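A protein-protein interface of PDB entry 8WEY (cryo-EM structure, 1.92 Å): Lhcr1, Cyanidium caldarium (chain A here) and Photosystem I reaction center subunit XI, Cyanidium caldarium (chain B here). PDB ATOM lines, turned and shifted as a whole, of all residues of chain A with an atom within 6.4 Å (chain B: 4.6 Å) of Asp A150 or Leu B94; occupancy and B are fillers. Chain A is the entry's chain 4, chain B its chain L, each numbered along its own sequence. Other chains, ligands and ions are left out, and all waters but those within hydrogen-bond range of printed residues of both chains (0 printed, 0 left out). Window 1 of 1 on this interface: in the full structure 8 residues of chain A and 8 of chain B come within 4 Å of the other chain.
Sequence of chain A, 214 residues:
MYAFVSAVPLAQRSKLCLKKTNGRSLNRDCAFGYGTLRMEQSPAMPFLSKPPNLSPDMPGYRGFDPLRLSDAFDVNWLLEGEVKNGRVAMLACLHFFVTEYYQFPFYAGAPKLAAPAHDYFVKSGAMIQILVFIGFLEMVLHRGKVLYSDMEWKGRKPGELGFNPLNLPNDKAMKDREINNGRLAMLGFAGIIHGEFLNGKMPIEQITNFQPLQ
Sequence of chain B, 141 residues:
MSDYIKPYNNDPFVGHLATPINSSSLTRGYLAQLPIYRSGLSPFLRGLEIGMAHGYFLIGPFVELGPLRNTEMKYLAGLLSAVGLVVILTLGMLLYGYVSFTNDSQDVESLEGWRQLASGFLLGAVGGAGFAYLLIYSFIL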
ATOM      1  N   MET A 139       7.263  31.709 -11.505  1.00  0.00           N
ATOM      2  CA  MET A 139       6.831  30.410 -10.916  1.00  0.00           C
ATOM      3  C   MET A 139       7.637  30.108  -9.639  1.00  0.00           C
ATOM      4  O   MET A 139       7.037  29.595  -8.667  1.00  0.00           O
ATOM      5  CB  MET A 139       7.026  29.265 -11.914  1.00  0.00           C
ATOM      6  CG  MET A 139       6.085  29.312 -13.106  1.00  0.00           C
ATOM      7  SD  MET A 139       4.340  29.003 -12.709  1.00  0.00           S
ATOM      8  CE  MET A 139       4.457  27.537 -11.688  1.00  0.00           C
ATOM      9  N   GLY A 144       4.587  28.444  -7.331  1.00  0.00           N
ATOM     10  CA  GLY A 144       3.473  27.728  -7.986  1.00  0.00           C
ATOM     11  C   GLY A 144       2.170  28.509  -7.981  1.00  0.00           C
ATOM     12  O   GLY A 144       1.501  28.513  -9.030  1.00  0.00           O
ATOM     13  N   LYS A 145       1.803  29.119  -6.848  1.00  0.00           N
ATOM     14  CA  LYS A 145       0.532  29.888  -6.692  1.00  0.00           C
ATOM     15  C   LYS A 145       0.687  31.235  -7.414  1.00  0.00           C
ATOM     16  O   LYS A 145       1.047  32.229  -6.755  1.00  0.00           O
ATOM     17  CB  LYS A 145       0.080  30.034  -5.229  1.00  0.00           C
ATOM     18  CG  LYS A 145       1.120  30.002  -4.109  1.00  0.00           C
ATOM     19  CD  LYS A 145       1.252  28.650  -3.425  1.00  0.00           C
ATOM     20  CE  LYS A 145       1.855  28.737  -2.038  1.00  0.00           C
ATOM     21  NZ  LYS A 145       3.294  29.073  -2.086  1.00  0.00           N
ATOM     22  N   VAL A 146       0.420  31.240  -8.727  1.00  0.00           N
ATOM     23  CA  VAL A 146       0.653  32.387  -9.658  1.00  0.00           C
ATOM     24  C   VAL A 146      -0.674  33.068 -10.025  1.00  0.00           C
ATOM     25  O   VAL A 146      -0.622  34.248 -10.409  1.00  0.00           O
ATOM     26  CB  VAL A 146       1.418  31.946 -10.924  1.00  0.00           C
ATOM     27  CG1 VAL A 146       2.891  31.684 -10.627  1.00  0.00           C
ATOM     28  CG2 VAL A 146       0.783  30.748 -11.620  1.00  0.00           C
ATOM     29  N   LEU A 147      -1.809  32.364  -9.944  1.00  0.00           N
ATOM     30  CA  LEU A 147      -3.140  32.884 -10.369  1.00  0.00           C
ATOM     31  C   LEU A 147      -3.679  33.841  -9.301  1.00  0.00           C
ATOM     32  O   LEU A 147      -3.308  33.683  -8.125  1.00  0.00           O
ATOM     33  CB  LEU A 147      -4.109  31.716 -10.587  1.00  0.00           C
ATOM     34  CG  LEU A 147      -3.666  30.642 -11.583  1.00  0.00           C
ATOM     35  CD1 LEU A 147      -4.734  29.568 -11.723  1.00  0.00           C
ATOM     36  CD2 LEU A 147      -3.335  31.249 -12.939  1.00  0.00           C
ATOM     37  N   TYR A 148      -4.539  34.784  -9.700  1.00  0.00           N
ATOM     38  CA  TYR A 148      -5.303  35.692  -8.799  1.00  0.00           C
ATOM     39  C   TYR A 148      -6.181  34.846  -7.859  1.00  0.00           C
ATOM     40  O   TYR A 148      -6.369  35.255  -6.697  1.00  0.00           O
ATOM     41  CB  TYR A 148      -6.086  36.710  -9.639  1.00  0.00           C
ATOM     42  CG  TYR A 148      -7.033  37.636  -8.909  1.00  0.00           C
ATOM     43  CD1 TYR A 148      -6.579  38.407  -7.855  1.00  0.00           C
ATOM     44  CD2 TYR A 148      -8.370  37.785  -9.282  1.00  0.00           C
ATOM     45  CE1 TYR A 148      -7.395  39.315  -7.198  1.00  0.00           C
ATOM     46  CE2 TYR A 148      -9.213  38.666  -8.621  1.00  0.00           C
ATOM     47  CZ  TYR A 148      -8.722  39.440  -7.578  1.00  0.00           C
ATOM     48  OH  TYR A 148      -9.508  40.332  -6.903  1.00  0.00           O
ATOM     49  N   SER A 149      -6.673  33.694  -8.331  1.00  0.00           N
ATOM     50  CA  SER A 149      -7.466  32.716  -7.540  1.00  0.00           C
ATOM     51  C   SER A 149      -6.572  31.954  -6.546  1.00  0.00           C
ATOM     52  O   SER A 149      -7.069  31.650  -5.444  1.00  0.00           O
ATOM     53  CB  SER A 149      -8.218  31.764  -8.444  1.00  0.00           C
ATOM     54  OG  SER A 149      -7.342  31.131  -9.366  1.00  0.00           O
ATOM     55  N   ASP A 150      -5.315  31.667  -6.915  1.00  0.00           N
ATOM     56  CA  ASP A 150      -4.397  30.742  -6.191  1.00  0.00           C
ATOM     57  C   ASP A 150      -3.463  31.512  -5.246  1.00  0.00           C
ATOM     58  O   ASP A 150      -3.259  31.019  -4.123  1.00  0.00           O
ATOM     59  CB  ASP A 150      -3.569  29.901  -7.169  1.00  0.00           C
ATOM     60  CG  ASP A 150      -4.371  28.872  -7.950  1.00  0.00           C
ATOM     61  OD1 ASP A 150      -5.613  28.992  -7.987  1.00  0.00           O
ATOM     62  OD2 ASP A 150      -3.745  27.955  -8.517  1.00  0.00           O
ATOM     63  N   MET A 151      -2.893  32.639  -5.692  1.00  0.00           N
ATOM     64  CA  MET A 151      -1.842  33.410  -4.963  1.00  0.00           C
ATOM     65  C   MET A 151      -2.344  33.754  -3.553  1.00  0.00           C
ATOM     66  O   MET A 151      -3.453  34.324  -3.448  1.00  0.00           O
ATOM     67  CB  MET A 151      -1.468  34.704  -5.695  1.00  0.00           C
ATOM     68  CG  MET A 151      -0.238  35.389  -5.112  1.00  0.00           C
ATOM     69  SD  MET A 151       0.456  36.675  -6.197  1.00  0.00           S
ATOM     70  CE  MET A 151       0.981  35.669  -7.584  1.00  0.00           C
ATOM     71  N   GLU A 152      -1.551  33.422  -2.528  1.00  0.00           N
ATOM     72  CA  GLU A 152      -1.919  33.559  -1.090  1.00  0.00           C
ATOM     73  C   GLU A 152      -0.773  34.234  -0.332  1.00  0.00           C
ATOM     74  O   GLU A 152       0.375  34.191  -0.825  1.00  0.00           O
ATOM     75  CB  GLU A 152      -2.292  32.201  -0.484  1.00  0.00           C
ATOM     76  CG  GLU A 152      -1.205  31.143  -0.572  1.00  0.00           C
ATOM     77  CD  GLU A 152      -1.655  29.730  -0.219  1.00  0.00           C
ATOM     78  OE1 GLU A 152      -2.777  29.570   0.312  1.00  0.00           O
ATOM     79  OE2 GLU A 152      -0.905  28.785  -0.533  1.00  0.00           O
ATOM     80  N   THR B  90      -1.065  23.128 -17.631  1.00  0.00           N
ATOM     81  CA  THR B  90      -0.737  23.535 -16.237  1.00  0.00           C
ATOM     82  C   THR B  90      -1.825  24.467 -15.687  1.00  0.00           C
ATOM     83  O   THR B  90      -2.228  24.268 -14.529  1.00  0.00           O
ATOM     84  CB  THR B  90       0.641  24.197 -16.150  1.00  0.00           C
ATOM     85  OG1 THR B  90       1.548  23.334 -16.835  1.00  0.00           O
ATOM     86  CG2 THR B  90       1.092  24.430 -14.724  1.00  0.00           C
ATOM     87  N   LEU B  91      -2.261  25.459 -16.466  1.00  0.00           N
ATOM     88  CA  LEU B  91      -3.390  26.350 -16.085  1.00  0.00           C
ATOM     89  C   LEU B  91      -4.635  25.484 -15.848  1.00  0.00           C
ATOM     90  O   LEU B  91      -5.326  25.709 -14.837  1.00  0.00           O
ATOM     91  CB  LEU B  91      -3.633  27.398 -17.177  1.00  0.00           C
ATOM     92  CG  LEU B  91      -4.916  28.222 -17.036  1.00  0.00           C
ATOM     93  CD1 LEU B  91      -4.977  28.934 -15.694  1.00  0.00           C
ATOM     94  CD2 LEU B  91      -5.046  29.222 -18.176  1.00  0.00           C
ATOM     95  N   GLY B  92      -4.904  24.538 -16.753  1.00  0.00           N
ATOM     96  CA  GLY B  92      -5.984  23.544 -16.613  1.00  0.00           C
ATOM     97  C   GLY B  92      -5.858  22.790 -15.303  1.00  0.00           C
ATOM     98  O   GLY B  92      -6.864  22.707 -14.573  1.00  0.00           O
ATOM     99  N   MET B  93      -4.655  22.284 -15.009  1.00  0.00           N
ATOM    100  CA  MET B  93      -4.328  21.584 -13.740  1.00  0.00           C
ATOM    101  C   MET B  93      -4.685  22.495 -12.567  1.00  0.00           C
ATOM    102  O   MET B  93      -5.393  22.032 -11.659  1.00  0.00           O
ATOM    103  CB  MET B  93      -2.844  21.216 -13.646  1.00  0.00           C
ATOM    104  CG  MET B  93      -2.474  20.015 -14.467  1.00  0.00           C
ATOM    105  SD  MET B  93      -0.763  19.498 -14.190  1.00  0.00           S
ATOM    106  CE  MET B  93      -0.931  18.700 -12.596  1.00  0.00           C
ATOM    107  N   LEU B  94      -4.222  23.744 -12.592  1.00  0.00           N
ATOM    108  CA  LEU B  94      -4.394  24.691 -11.461  1.00  0.00           C
ATOM    109  C   LEU B  94      -5.885  24.925 -11.216  1.00  0.00           C
ATOM    110  O   LEU B  94      -6.295  24.839 -10.048  1.00  0.00           O
ATOM    111  CB  LEU B  94      -3.645  25.995 -11.746  1.00  0.00           C
ATOM    112  CG  LEU B  94      -2.123  25.895 -11.670  1.00  0.00           C
ATOM    113  CD1 LEU B  94      -1.482  27.188 -12.135  1.00  0.00           C
ATOM    114  CD2 LEU B  94      -1.659  25.538 -10.263  1.00  0.00           C
ATOM    115  N   LEU B  95      -6.653  25.185 -12.277  1.00  0.00           N
ATOM    116  CA  LEU B  95      -8.126  25.409 -12.219  1.00  0.00           C
ATOM    117  C   LEU B  95      -8.817  24.187 -11.605  1.00  0.00           C
ATOM    118  O   LEU B  95      -9.621  24.380 -10.675  1.00  0.00           O
ATOM    119  CB  LEU B  95      -8.659  25.691 -13.629  1.00  0.00           C
ATOM    120  CG  LEU B  95      -8.368  27.085 -14.175  1.00  0.00           C
ATOM    121  CD1 LEU B  95      -8.799  27.184 -15.628  1.00  0.00           C
ATOM    122  CD2 LEU B  95      -9.057  28.151 -13.340  1.00  0.00           C
ATOM    123  N   TYR B  96      -8.514  22.984 -12.098  1.00  0.00           N
ATOM    124  CA  TYR B  96      -9.052  21.710 -11.557  1.00  0.00           C
ATOM    125  C   TYR B  96      -8.844  21.661 -10.035  1.00  0.00           C
ATOM    126  O   TYR B  96      -9.833  21.492  -9.296  1.00  0.00           O
ATOM    127  CB  TYR B  96      -8.399  20.492 -12.205  1.00  0.00           C
ATOM    128  CG  TYR B  96      -8.896  19.196 -11.622  1.00  0.00           C
ATOM    129  CD1 TYR B  96     -10.090  18.641 -12.054  1.00  0.00           C
ATOM    130  CD2 TYR B  96      -8.218  18.572 -10.585  1.00  0.00           C
ATOM    131  CE1 TYR B  96     -10.581  17.471 -11.493  1.00  0.00           C
ATOM    132  CE2 TYR B  96      -8.689  17.398 -10.021  1.00  0.00           C
ATOM    133  CZ  TYR B  96      -9.875  16.847 -10.478  1.00  0.00           C
ATOM    134  OH  TYR B  96     -10.356  15.698  -9.922  1.00  0.00           O
ATOM    135  N   GLY B  97      -7.596  21.822  -9.591  1.00  0.00           N
ATOM    136  CA  GLY B  97      -7.201  21.758  -8.172  1.00  0.00           C
ATOM    137  C   GLY B  97      -7.951  22.767  -7.317  1.00  0.00           C
ATOM    138  O   GLY B  97      -8.393  22.390  -6.208  1.00  0.00           O
ATOM    139  N   TYR B  98      -8.087  24.004  -7.804  1.00  0.00           N
ATOM    140  CA  TYR B  98      -8.725  25.128  -7.074  1.00  0.00           C
ATOM    141  C   TYR B  98     -10.193  24.787  -6.823  1.00  0.00           C
ATOM    142  O   TYR B  98     -10.676  24.973  -5.693  1.00  0.00           O
ATOM    143  CB  TYR B  98      -8.604  26.439  -7.855  1.00  0.00           C
ATOM    144  CG  TYR B  98      -9.123  27.640  -7.105  1.00  0.00           C
ATOM    145  CD1 TYR B  98      -8.509  28.067  -5.936  1.00  0.00           C
ATOM    146  CD2 TYR B  98     -10.240  28.338  -7.541  1.00  0.00           C
ATOM    147  CE1 TYR B  98      -8.983  29.159  -5.225  1.00  0.00           C
ATOM    148  CE2 TYR B  98     -10.724  29.434  -6.843  1.00  0.00           C
ATOM    149  CZ  TYR B  98     -10.094  29.847  -5.682  1.00  0.00           C
ATOM    150  OH  TYR B  98     -10.573  30.925  -4.995  1.00  0.00           O
ATOM    151  N   ARG B 115      -1.135  21.943  -6.438  1.00  0.00           N
ATOM    152  CA  ARG B 115      -0.369  23.130  -6.922  1.00  0.00           C
ATOM    153  C   ARG B 115       1.121  22.782  -7.049  1.00  0.00           C
ATOM    154  O   ARG B 115       1.748  23.235  -8.026  1.00  0.00           O
ATOM    155  CB  ARG B 115      -0.568  24.343  -6.006  1.00  0.00           C
ATOM    156  CG  ARG B 115      -1.870  25.097  -6.249  1.00  0.00           C
ATOM    157  CD  ARG B 115      -1.809  26.539  -5.782  1.00  0.00           C
ATOM    158  NE  ARG B 115      -1.922  26.652  -4.329  1.00  0.00           N
ATOM    159  CZ  ARG B 115      -2.930  27.209  -3.649  1.00  0.00           C
ATOM    160  NH1 ARG B 115      -3.976  27.745  -4.265  1.00  0.00           N
ATOM    161  NH2 ARG B 115      -2.885  27.227  -2.327  1.00  0.00           N
ATOM    162  N   ALA B 118       1.424  20.502 -10.043  1.00  0.00           N
ATOM    163  CA  ALA B 118       1.284  21.373 -11.232  1.00  0.00           C
ATOM    164  C   ALA B 118       2.620  22.068 -11.515  1.00  0.00           C
ATOM    165  O   ALA B 118       3.029  22.099 -12.694  1.00  0.00           O
ATOM    166  CB  ALA B 118       0.173  22.375 -11.019  1.00  0.00           C
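Of chain B, only Leu B94, Tyr B98 and Arg B115 come within 4 Å of Asp A150. Of chain A, only Leu A147 and Asp A150 come within 4 Å of Leu B94. Printed residues of chain A within 4 Å of Leu B91: Leu A147 (3.96 Å). Of the printed residues of chain B, Lys A145 touches Arg B115 (3.9 Å). Printed residues of chain A within 4 Å of Tyr B98: Ser A149 and Asp A150. The nearest residue of chain A that does not touch Leu B94 is Val A146 (4.3 Å). The nearest printed residue of chain B that does not touch Lys A145 is Leu B94 (6.0 Å).
Arg B115 touches Lys A145. Leu A147 touches Leu B91. Leu B94 touches Leu A147. CE1 of Tyr B98 touches O of Ser A149, at 3.1 Å. OD2 of Asp A150 touches CD2 of Leu B94, 3.6 Å away. OD1 of Asp A150 touches CD1 of Tyr B98 (3.7 Å).
The side-chain hydroxyl of Ser A149 sits at hydrogen-bond distance from the side-chain carboxylate of Asp A150 (3.1 Å).
Of the 10 printed residues of chain A, 5 touch a printed residue of chain B. Printed residues of chain A that touch a printed residue of chain B: Lys A145, Leu A147, Ser A149, Asp A150 and Glu A152. Along chain A the printed residues that touch a printed residue of chain B span positions 145 to 152. Of the 11 printed residues of chain B, 4 touch a printed residue of chain A. Printed residues of chain B that touch a printed residue of chain A: Leu B91, Leu B94, Tyr B98 and Arg B115. Among the printed residues, Asp or Glu carboxylates within 4 Å of a Lys or Arg side-chain nitrogen of the other chain: Glu A152 with Arg B115 (3.1 Å).
O of Asp A150 lies within hydrogen-bond range of NH1 of Arg B115, at 3.4 Å. The side-chain carboxylate (OE2) of Glu A152 is in salt-bridge range of the guanidinium group (NH2) of Arg B115, at 3.1 Å.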
